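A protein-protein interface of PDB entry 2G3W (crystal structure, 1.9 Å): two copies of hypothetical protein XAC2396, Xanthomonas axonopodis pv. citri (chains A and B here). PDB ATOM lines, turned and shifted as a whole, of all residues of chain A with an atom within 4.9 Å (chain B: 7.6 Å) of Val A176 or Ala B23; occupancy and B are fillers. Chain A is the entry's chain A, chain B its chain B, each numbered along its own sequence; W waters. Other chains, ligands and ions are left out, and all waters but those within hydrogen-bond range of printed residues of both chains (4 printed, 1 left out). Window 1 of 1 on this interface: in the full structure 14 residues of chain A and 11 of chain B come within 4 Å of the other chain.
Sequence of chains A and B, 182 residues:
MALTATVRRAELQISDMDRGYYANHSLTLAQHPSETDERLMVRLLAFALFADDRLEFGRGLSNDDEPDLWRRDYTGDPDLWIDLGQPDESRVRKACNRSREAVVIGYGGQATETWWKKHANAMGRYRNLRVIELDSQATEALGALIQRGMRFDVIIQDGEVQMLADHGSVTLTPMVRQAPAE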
ATOM      1  N   TRP A 116     -18.200  22.823 -11.409  1.00  0.00           N
ATOM      2  CA  TRP A 116     -19.098  22.912 -12.567  1.00  0.00           C
ATOM      3  C   TRP A 116     -18.574  22.194 -13.803  1.00  0.00           C
ATOM      4  O   TRP A 116     -19.249  21.348 -14.369  1.00  0.00           O
ATOM      5  CB  TRP A 116     -19.466  24.368 -12.903  1.00  0.00           C
ATOM      6  CG  TRP A 116     -20.307  24.386 -14.147  1.00  0.00           C
ATOM      7  CD1 TRP A 116     -19.903  24.676 -15.424  1.00  0.00           C
ATOM      8  CD2 TRP A 116     -21.667  23.975 -14.232  1.00  0.00           C
ATOM      9  NE1 TRP A 116     -20.978  24.524 -16.300  1.00  0.00           N
ATOM     10  CE2 TRP A 116     -22.057  24.065 -15.587  1.00  0.00           C
ATOM     11  CE3 TRP A 116     -22.609  23.543 -13.280  1.00  0.00           C
ATOM     12  CZ2 TRP A 116     -23.368  23.761 -16.015  1.00  0.00           C
ATOM     13  CZ3 TRP A 116     -23.904  23.218 -13.710  1.00  0.00           C
ATOM     14  CH2 TRP A 116     -24.262  23.325 -15.076  1.00  0.00           C
ATOM     15  N   ARG A 130     -31.742  24.214 -10.532  1.00  0.00           N
ATOM     16  CA  ARG A 130     -31.161  25.530 -10.790  1.00  0.00           C
ATOM     17  C   ARG A 130     -29.778  25.602 -10.130  1.00  0.00           C
ATOM     18  O   ARG A 130     -29.636  25.313  -8.938  1.00  0.00           O
ATOM     19  CB  ARG A 130     -32.096  26.629 -10.211  1.00  0.00           C
ATOM     20  CG  ARG A 130     -31.585  28.061 -10.391  1.00  0.00           C
ATOM     21  CD  ARG A 130     -32.586  29.078  -9.727  1.00  0.00           C
ATOM     22  NE  ARG A 130     -33.843  29.009 -10.460  1.00  0.00           N
ATOM     23  CZ  ARG A 130     -34.084  29.608 -11.626  1.00  0.00           C
ATOM     24  NH1 ARG A 130     -33.163  30.365 -12.228  1.00  0.00           N
ATOM     25  NH2 ARG A 130     -35.241  29.427 -12.201  1.00  0.00           N
ATOM     26  N   VAL A 131     -28.742  25.946 -10.885  1.00  0.00           N
ATOM     27  CA  VAL A 131     -27.416  26.066 -10.305  1.00  0.00           C
ATOM     28  C   VAL A 131     -26.983  27.490 -10.527  1.00  0.00           C
ATOM     29  O   VAL A 131     -27.050  28.013 -11.658  1.00  0.00           O
ATOM     30  CB  VAL A 131     -26.364  25.070 -10.926  1.00  0.00           C
ATOM     31  CG1 VAL A 131     -24.940  25.335 -10.289  1.00  0.00           C
ATOM     32  CG2 VAL A 131     -26.794  23.626 -10.693  1.00  0.00           C
ATOM     33  N   ILE A 132     -26.622  28.155  -9.432  1.00  0.00           N
ATOM     34  CA  ILE A 132     -26.068  29.497  -9.536  1.00  0.00           C
ATOM     35  C   ILE A 132     -24.706  29.610  -8.853  1.00  0.00           C
ATOM     36  O   ILE A 132     -24.384  28.847  -7.912  1.00  0.00           O
ATOM     37  CB  ILE A 132     -27.020  30.595  -9.038  1.00  0.00           C
ATOM     38  CG1 ILE A 132     -27.091  30.640  -7.549  1.00  0.00           C
ATOM     39  CG2 ILE A 132     -28.472  30.502  -9.672  1.00  0.00           C
ATOM     40  CD1 ILE A 132     -27.482  32.002  -7.090  1.00  0.00           C
ATOM     41  N   PRO A 174     -25.302  37.204  -9.887  1.00  0.00           N
ATOM     42  CA  PRO A 174     -25.245  35.738  -9.813  1.00  0.00           C
ATOM     43  C   PRO A 174     -25.151  35.128 -11.196  1.00  0.00           C
ATOM     44  O   PRO A 174     -25.761  35.634 -12.144  1.00  0.00           O
ATOM     45  CB  PRO A 174     -26.546  35.366  -9.124  1.00  0.00           C
ATOM     46  CG  PRO A 174     -26.897  36.653  -8.302  1.00  0.00           C
ATOM     47  CD  PRO A 174     -26.509  37.745  -9.245  1.00  0.00           C
ATOM     48  N   MET A 175     -24.326  34.107 -11.332  1.00  0.00           N
ATOM     49  CA  MET A 175     -24.182  33.451 -12.610  1.00  0.00           C
ATOM     50  C   MET A 175     -25.085  32.202 -12.652  1.00  0.00           C
ATOM     51  O   MET A 175     -24.974  31.325 -11.829  1.00  0.00           O
ATOM     52  CB  MET A 175     -22.690  33.159 -12.934  1.00  0.00           C
ATOM     53  CG  MET A 175     -22.477  32.117 -14.031  1.00  0.00           C
ATOM     54  SD  MET A 175     -23.032  32.762 -15.779  1.00  0.00           S
ATOM     55  CE  MET A 175     -22.929  30.978 -16.724  1.00  0.00           C
ATOM     56  N   VAL A 176     -25.982  32.142 -13.629  1.00  0.00           N
ATOM     57  CA  VAL A 176     -26.873  30.992 -13.732  1.00  0.00           C
ATOM     58  C   VAL A 176     -26.213  29.898 -14.604  1.00  0.00           C
ATOM     59  O   VAL A 176     -26.122  30.045 -15.820  1.00  0.00           O
ATOM     60  CB  VAL A 176     -28.235  31.403 -14.280  1.00  0.00           C
ATOM     61  CG1 VAL A 176     -29.173  30.211 -14.298  1.00  0.00           C
ATOM     62  CG2 VAL A 176     -28.830  32.548 -13.408  1.00  0.00           C
ATOM     63  N   ARG A 177     -25.704  28.843 -13.971  1.00  0.00           N
ATOM     64  CA  ARG A 177     -25.149  27.693 -14.675  1.00  0.00           C
ATOM     65  C   ARG A 177     -26.223  26.792 -15.271  1.00  0.00           C
ATOM     66  O   ARG A 177     -25.995  26.131 -16.256  1.00  0.00           O
ATOM     67  CB  ARG A 177     -24.292  26.855 -13.705  1.00  0.00           C
ATOM     68  CG  ARG A 177     -23.136  27.627 -13.053  1.00  0.00           C
ATOM     69  CD  ARG A 177     -22.005  27.840 -14.033  1.00  0.00           C
ATOM     70  NE  ARG A 177     -20.766  28.309 -13.369  1.00  0.00           N
ATOM     71  CZ  ARG A 177     -19.718  28.801 -14.025  1.00  0.00           C
ATOM     72  NH1 ARG A 177     -19.756  28.904 -15.349  1.00  0.00           N
ATOM     73  NH2 ARG A 177     -18.624  29.196 -13.373  1.00  0.00           N
ATOM     74  N   GLN A 178     -27.385  26.714 -14.638  1.00  0.00           N
ATOM     75  CA  GLN A 178     -28.454  25.857 -15.139  1.00  0.00           C
ATOM     76  C   GLN A 178     -29.750  26.378 -14.567  1.00  0.00           C
ATOM     77  O   GLN A 178     -29.748  26.805 -13.432  1.00  0.00           O
ATOM     78  CB  GLN A 178     -28.236  24.417 -14.661  1.00  0.00           C
ATOM     79  CG  GLN A 178     -29.160  23.411 -15.371  1.00  0.00           C
ATOM     80  CD  GLN A 178     -28.734  21.958 -15.229  1.00  0.00           C
ATOM     81  OE1 GLN A 178     -27.563  21.643 -15.353  1.00  0.00           O
ATOM     82  NE2 GLN A 178     -29.706  21.063 -15.024  1.00  0.00           N
ATOM     83  N   ALA A 179     -30.839  26.368 -15.338  1.00  0.00           N
ATOM     84  CA  ALA A 179     -32.149  26.727 -14.790  1.00  0.00           C
ATOM     85  C   ALA A 179     -33.190  25.751 -15.324  1.00  0.00           C
ATOM     86  O   ALA A 179     -33.023  25.260 -16.437  1.00  0.00           O
ATOM     87  CB  ALA A 179     -32.505  28.173 -15.159  1.00  0.00           C
ATOM     88  N   LEU B  12     -28.718  22.550 -24.516  1.00  0.00           N
ATOM     89  CA  LEU B  12     -27.357  22.878 -24.924  1.00  0.00           C
ATOM     90  C   LEU B  12     -26.428  22.797 -23.717  1.00  0.00           C
ATOM     91  O   LEU B  12     -26.732  23.370 -22.684  1.00  0.00           O
ATOM     92  CB  LEU B  12     -27.279  24.284 -25.498  1.00  0.00           C
ATOM     93  CG  LEU B  12     -28.120  24.626 -26.751  1.00  0.00           C
ATOM     94  CD1 LEU B  12     -27.809  26.053 -27.192  1.00  0.00           C
ATOM     95  CD2 LEU B  12     -27.882  23.633 -27.894  1.00  0.00           C
ATOM     96  N   GLN B  13     -25.302  22.100 -23.861  1.00  0.00           N
ATOM     97  CA  GLN B  13     -24.275  22.127 -22.834  1.00  0.00           C
ATOM     98  C   GLN B  13     -23.091  22.924 -23.384  1.00  0.00           C
ATOM     99  O   GLN B  13     -22.328  22.441 -24.239  1.00  0.00           O
ATOM    100  CB  GLN B  13     -23.927  20.725 -22.392  1.00  0.00           C
ATOM    101  CG  GLN B  13     -25.095  19.759 -22.598  1.00  0.00           C
ATOM    102  CD  GLN B  13     -25.904  19.417 -21.378  1.00  0.00           C
ATOM    103  OE1 GLN B  13     -26.993  19.958 -21.187  1.00  0.00           O
ATOM    104  NE2 GLN B  13     -25.417  18.444 -20.581  1.00  0.00           N
ATOM    105  N   ILE B  14     -22.974  24.155 -22.933  1.00  0.00           N
ATOM    106  CA  ILE B  14     -22.041  25.096 -23.549  1.00  0.00           C
ATOM    107  C   ILE B  14     -20.704  25.219 -22.784  1.00  0.00           C
ATOM    108  O   ILE B  14     -20.683  25.562 -21.594  1.00  0.00           O
ATOM    109  CB  ILE B  14     -22.679  26.480 -23.696  1.00  0.00           C
ATOM    110  CG1 ILE B  14     -23.967  26.392 -24.547  1.00  0.00           C
ATOM    111  CG2 ILE B  14     -21.697  27.464 -24.319  1.00  0.00           C
ATOM    112  CD1 ILE B  14     -24.697  27.706 -24.691  1.00  0.00           C
ATOM    113  N   SER B  15     -19.598  24.972 -23.486  1.00  0.00           N
ATOM    114  CA  SER B  15     -18.281  25.303 -22.951  1.00  0.00           C
ATOM    115  C   SER B  15     -17.645  26.284 -23.912  1.00  0.00           C
ATOM    116  O   SER B  15     -17.172  25.907 -24.990  1.00  0.00           O
ATOM    117  CB  SER B  15     -17.417  24.048 -22.803  1.00  0.00           C
ATOM    118  OG  SER B  15     -18.131  23.112 -22.018  1.00  0.00           O
ATOM    119  N   ASP B  16     -17.672  27.556 -23.548  1.00  0.00           N
ATOM    120  CA  ASP B  16     -17.143  28.590 -24.439  1.00  0.00           C
ATOM    121  C   ASP B  16     -15.880  29.167 -23.824  1.00  0.00           C
ATOM    122  O   ASP B  16     -15.958  30.025 -22.941  1.00  0.00           O
ATOM    123  CB  ASP B  16     -18.226  29.672 -24.738  1.00  0.00           C
ATOM    124  CG  ASP B  16     -17.733  30.776 -25.682  1.00  0.00           C
ATOM    125  OD1 ASP B  16     -16.506  30.972 -25.790  1.00  0.00           O
ATOM    126  OD2 ASP B  16     -18.576  31.465 -26.312  1.00  0.00           O
ATOM    127  N   GLY B  20     -15.292  32.602 -21.877  1.00  0.00           N
ATOM    128  CA  GLY B  20     -15.265  32.034 -20.525  1.00  0.00           C
ATOM    129  C   GLY B  20     -16.679  31.773 -19.973  1.00  0.00           C
ATOM    130  O   GLY B  20     -16.948  31.959 -18.784  1.00  0.00           O
ATOM    131  N   TYR B  21     -17.583  31.340 -20.844  1.00  0.00           N
ATOM    132  CA  TYR B  21     -18.972  31.071 -20.515  1.00  0.00           C
ATOM    133  C   TYR B  21     -19.243  29.563 -20.497  1.00  0.00           C
ATOM    134  O   TYR B  21     -18.976  28.841 -21.505  1.00  0.00           O
ATOM    135  CB  TYR B  21     -19.914  31.776 -21.504  1.00  0.00           C
ATOM    136  CG  TYR B  21     -21.398  31.570 -21.213  1.00  0.00           C
ATOM    137  CD1 TYR B  21     -22.056  32.357 -20.255  1.00  0.00           C
ATOM    138  CD2 TYR B  21     -22.130  30.562 -21.873  1.00  0.00           C
ATOM    139  CE1 TYR B  21     -23.428  32.160 -19.969  1.00  0.00           C
ATOM    140  CE2 TYR B  21     -23.494  30.360 -21.589  1.00  0.00           C
ATOM    141  CZ  TYR B  21     -24.127  31.205 -20.649  1.00  0.00           C
ATOM    142  OH  TYR B  21     -25.449  31.011 -20.351  1.00  0.00           O
ATOM    143  N   TYR B  22     -19.734  29.076 -19.349  1.00  0.00           N
ATOM    144  CA  TYR B  22     -20.007  27.620 -19.149  1.00  0.00           C
ATOM    145  C   TYR B  22     -21.379  27.541 -18.506  1.00  0.00           C
ATOM    146  O   TYR B  22     -21.575  28.130 -17.429  1.00  0.00           O
ATOM    147  CB  TYR B  22     -18.961  27.004 -18.211  1.00  0.00           C
ATOM    148  CG  TYR B  22     -17.556  27.210 -18.743  1.00  0.00           C
ATOM    149  CD1 TYR B  22     -17.004  26.321 -19.663  1.00  0.00           C
ATOM    150  CD2 TYR B  22     -16.808  28.319 -18.355  1.00  0.00           C
ATOM    151  CE1 TYR B  22     -15.733  26.519 -20.164  1.00  0.00           C
ATOM    152  CE2 TYR B  22     -15.537  28.542 -18.861  1.00  0.00           C
ATOM    153  CZ  TYR B  22     -15.011  27.635 -19.756  1.00  0.00           C
ATOM    154  OH  TYR B  22     -13.740  27.860 -20.254  1.00  0.00           O
ATOM    155  N   ALA B  23     -22.332  26.884 -19.164  1.00  0.00           N
ATOM    156  CA  ALA B  23     -23.725  26.780 -18.666  1.00  0.00           C
ATOM    157  C   ALA B  23     -24.452  25.722 -19.445  1.00  0.00           C
ATOM    158  O   ALA B  23     -24.074  25.432 -20.598  1.00  0.00           O
ATOM    159  CB  ALA B  23     -24.497  28.130 -18.875  1.00  0.00           C
ATOM    160  N   ASN B  24     -25.521  25.181 -18.854  1.00  0.00           N
ATOM    161  CA  ASN B  24     -26.445  24.296 -19.569  1.00  0.00           C
ATOM    162  C   ASN B  24     -27.755  25.083 -19.743  1.00  0.00           C
ATOM    163  O   ASN B  24     -28.115  25.817 -18.849  1.00  0.00           O
ATOM    164  CB  ASN B  24     -26.755  23.032 -18.777  1.00  0.00           C
ATOM    165  CG  ASN B  24     -25.593  22.143 -18.607  1.00  0.00           C
ATOM    166  OD1 ASN B  24     -24.666  22.154 -19.406  1.00  0.00           O
ATOM    167  ND2 ASN B  24     -25.628  21.327 -17.566  1.00  0.00           N
ATOM    168  N   HIS B  25     -28.430  24.923 -20.874  1.00  0.00           N
ATOM    169  CA  HIS B  25     -29.713  25.629 -21.213  1.00  0.00           C
ATOM    170  C   HIS B  25     -30.708  24.593 -21.720  1.00  0.00           C
ATOM    171  O   HIS B  25     -30.311  23.714 -22.490  1.00  0.00           O
ATOM    172  CB  HIS B  25     -29.482  26.642 -22.336  1.00  0.00           C
ATOM    173  CG  HIS B  25     -28.658  27.815 -21.920  1.00  0.00           C
ATOM    174  ND1 HIS B  25     -29.223  28.929 -21.345  1.00  0.00           N
ATOM    175  CD2 HIS B  25     -27.315  28.007 -21.872  1.00  0.00           C
ATOM    176  CE1 HIS B  25     -28.273  29.783 -21.002  1.00  0.00           C
ATOM    177  NE2 HIS B  25     -27.105  29.261 -21.328  1.00  0.00           N
ATOM    178  N   ALA B  51     -25.164  33.002 -25.630  1.00  0.00           N
ATOM    179  CA  ALA B  51     -25.966  32.492 -24.505  1.00  0.00           C
ATOM    180  C   ALA B  51     -25.827  33.301 -23.233  1.00  0.00           C
ATOM    181  O   ALA B  51     -24.730  33.683 -22.847  1.00  0.00           O
ATOM    182  CB  ALA B  51     -25.644  30.980 -24.228  1.00  0.00           C
ATOM    183  N   ASP B  52     -26.983  33.493 -22.577  1.00  0.00           N
ATOM    184  CA  ASP B  52     -27.145  34.201 -21.340  1.00  0.00           C
ATOM    185  C   ASP B  52     -28.476  33.707 -20.758  1.00  0.00           C
ATOM    186  O   ASP B  52     -29.367  33.319 -21.506  1.00  0.00           O
ATOM    187  CB  ASP B  52     -27.298  35.694 -21.656  1.00  0.00           C
ATOM    188  CG  ASP B  52     -27.438  36.515 -20.438  1.00  0.00           C
ATOM    189  OD1 ASP B  52     -26.427  36.731 -19.760  1.00  0.00           O
ATOM    190  OD2 ASP B  52     -28.560  36.920 -20.117  1.00  0.00           O
ATOM    191  N   ASP B  53     -28.634  33.760 -19.448  1.00  0.00           N
ATOM    192  CA  ASP B  53     -29.917  33.395 -18.837  1.00  0.00           C
ATOM    193  C   ASP B  53     -31.068  34.323 -19.280  1.00  0.00           C
ATOM    194  O   ASP B  53     -32.244  33.928 -19.263  1.00  0.00           O
ATOM    195  CB  ASP B  53     -29.784  33.377 -17.315  1.00  0.00           C
ATOM    196  CG  ASP B  53     -31.062  32.954 -16.626  1.00  0.00           C
ATOM    197  OD1 ASP B  53     -31.436  31.769 -16.753  1.00  0.00           O
ATOM    198  OD2 ASP B  53     -31.709  33.806 -15.998  1.00  0.00           O
ATOM    199  N   ARG B  54     -30.741  35.546 -19.677  1.00  0.00           N
ATOM    200  CA  ARG B  54     -31.770  36.540 -20.037  1.00  0.00           C
ATOM    201  C   ARG B  54     -31.944  36.738 -21.547  1.00  0.00           C
ATOM    202  O   ARG B  54     -32.694  37.621 -21.982  1.00  0.00           O
ATOM    203  CB  ARG B  54     -31.522  37.881 -19.321  1.00  0.00           C
ATOM    204  CG  ARG B  54     -31.146  37.682 -17.833  1.00  0.00           C
ATOM    205  CD  ARG B  54     -31.153  39.001 -17.008  1.00  0.00           C
ATOM    206  NE  ARG B  54     -32.449  39.675 -17.017  1.00  0.00           N
ATOM    207  CZ  ARG B  54     -33.500  39.346 -16.264  1.00  0.00           C
ATOM    208  NH1 ARG B  54     -33.439  38.326 -15.414  1.00  0.00           N
ATOM    209  NH2 ARG B  54     -34.630  40.038 -16.374  1.00  0.00           N
ATOM    210  N   PHE B 152     -27.391  19.029 -27.595  1.00  0.00           N
ATOM    211  CA  PHE B 152     -26.074  19.357 -28.146  1.00  0.00           C
ATOM    212  C   PHE B 152     -25.055  19.701 -27.085  1.00  0.00           C
ATOM    213  O   PHE B 152     -25.369  20.433 -26.141  1.00  0.00           O
ATOM    214  CB  PHE B 152     -26.166  20.526 -29.145  1.00  0.00           C
ATOM    215  CG  PHE B 152     -26.758  20.138 -30.471  1.00  0.00           C
ATOM    216  CD1 PHE B 152     -25.942  19.631 -31.497  1.00  0.00           C
ATOM    217  CD2 PHE B 152     -28.114  20.230 -30.683  1.00  0.00           C
ATOM    218  CE1 PHE B 152     -26.480  19.260 -32.723  1.00  0.00           C
ATOM    219  CE2 PHE B 152     -28.657  19.845 -31.918  1.00  0.00           C
ATOM    220  CZ  PHE B 152     -27.833  19.360 -32.931  1.00  0.00           C
ATOM    221  N   VAL B 154     -21.907  22.111 -26.980  1.00  0.00           N
ATOM    222  CA  VAL B 154     -21.376  23.195 -27.792  1.00  0.00           C
ATOM    223  C   VAL B 154     -20.024  23.564 -27.188  1.00  0.00           C
ATOM    224  O   VAL B 154     -19.930  24.015 -26.026  1.00  0.00           O
ATOM    225  CB  VAL B 154     -22.323  24.414 -27.849  1.00  0.00           C
ATOM    226  CG1 VAL B 154     -21.794  25.486 -28.761  1.00  0.00           C
ATOM    227  CG2 VAL B 154     -23.734  23.981 -28.309  1.00  0.00           C
HETATM  228  O   HOH W   1     -26.626  31.464 -18.129  1.00  0.00           O
HETATM  229  O   HOH W   2     -20.471  23.964 -19.327  1.00  0.00           O
HETATM  230  O   HOH W   3     -33.381  32.010 -14.527  1.00  0.00           O
HETATM  231  O   HOH W   4     -19.052  31.143 -17.331  1.00  0.00           O
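Of the 17 printed residues of chain B, 5 touch a printed residue of chain A.
Printed residues of chain B that touch a printed residue of chain A: Tyr B21, Tyr B22, Ala B23, Asn B24 and Asp B53.
Among the printed residues, 12 pairs touch across the chains.
Among the printed residues, no Asp or Glu carboxylate lies within 4 Å of a Lys or Arg side-chain nitrogen of the other chain.
Of the printed residues of chain B, Trp A116 touches Tyr B22 (3.7 Å), Ala B23 (3.95 Å) and Asn B24 (3.5 Å).
Val A131 touches none of the printed residues of chain B.
Of the printed residues of chain A, Tyr B22 touches Trp A116, Met A175 and Arg A177.
Of the printed residues of chain A, Ala B23 touches Trp A116 (3.95 Å), Met A175 (3.9 Å), Val A176 (3.95 Å) and Arg A177 (3.4 Å).
Asp B52 touches none of the printed residues of chain A.
The nearest residue of chain B that does not touch Val A176 is Tyr B21 (4.7 Å).
The guanidinium group of Arg A177 lies within hydrogen-bond range of the backbone carbonyl oxygen of Tyr B22, at 2.9 Å.
The backbone carbonyl oxygen of Arg A177 is in hydrogen-bond range of the backbone NH of Asn B24 (2.8 Å).
The side-chain amide nitrogen (ND2) of Asn B24 lies within hydrogen-bond range of the side-chain amide oxygen (OE1) of Gln A178.
Among the printed residues, merely in contact across the chains: Trp A116 with Tyr B22 (3.7 Å), Trp A116 with Ala B23 (3.95 Å), Trp A116 with Asn B24 (3.5 Å), Met A175 with Tyr B21 (3.5 Å), Met A175 with Tyr B22 (3.2 Å), Met A175 with Ala B23 (3.9 Å), Val A176 with Ala B23 (3.95 Å), Val A176 with Asp B53 (3.7 Å) and Arg A177 with Ala B23 (3.4 Å).
No position is printed for both chains.
Of the 12 pairs that touch across the chains among the printed residues, none has its exchanged pair printed and touching as well.
N of Arg A177 sits at hydrogen-bond distance from O of Val A131.
The backbone NH (N) of Val A131 lies within hydrogen-bond range of the backbone carbonyl oxygen (O) of Gln A178 (2.9 Å).
N of Ile B14 lies within hydrogen-bond range of O of Ala B23 (2.9 Å).
O of Tyr B21 is in hydrogen-bond range of N of Asp B16 (2.7 Å).
OH of Tyr B21 sits at hydrogen-bond distance from NE2 of His B25, at 2.6 Å.
Water W1 lies within hydrogen-bond range of the side-chain hydroxyl (OH) of Tyr B21 (2.6 Å), the backbone carbonyl oxygen (O) of Val A176 (2.8 Å) and the backbone NH (N) of Asp B53 (3.3 Å).
Water W4 lies within hydrogen-bond range of the backbone carbonyl oxygen of Gly B20, the backbone NH of Tyr B22 and the guanidinium group of Arg A177.
Water W2 lies within hydrogen-bond range of the backbone carbonyl oxygen of Ile B14 (2.8 Å), the indole nitrogen of Trp A116 (3.1 Å) and the backbone NH of Ala B23 (3.5 Å).
Water W3 lies within hydrogen-bond range of the guanidinium group (NH1) of Arg A130 and the side-chain carboxylate (OD2) of Asp B53.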
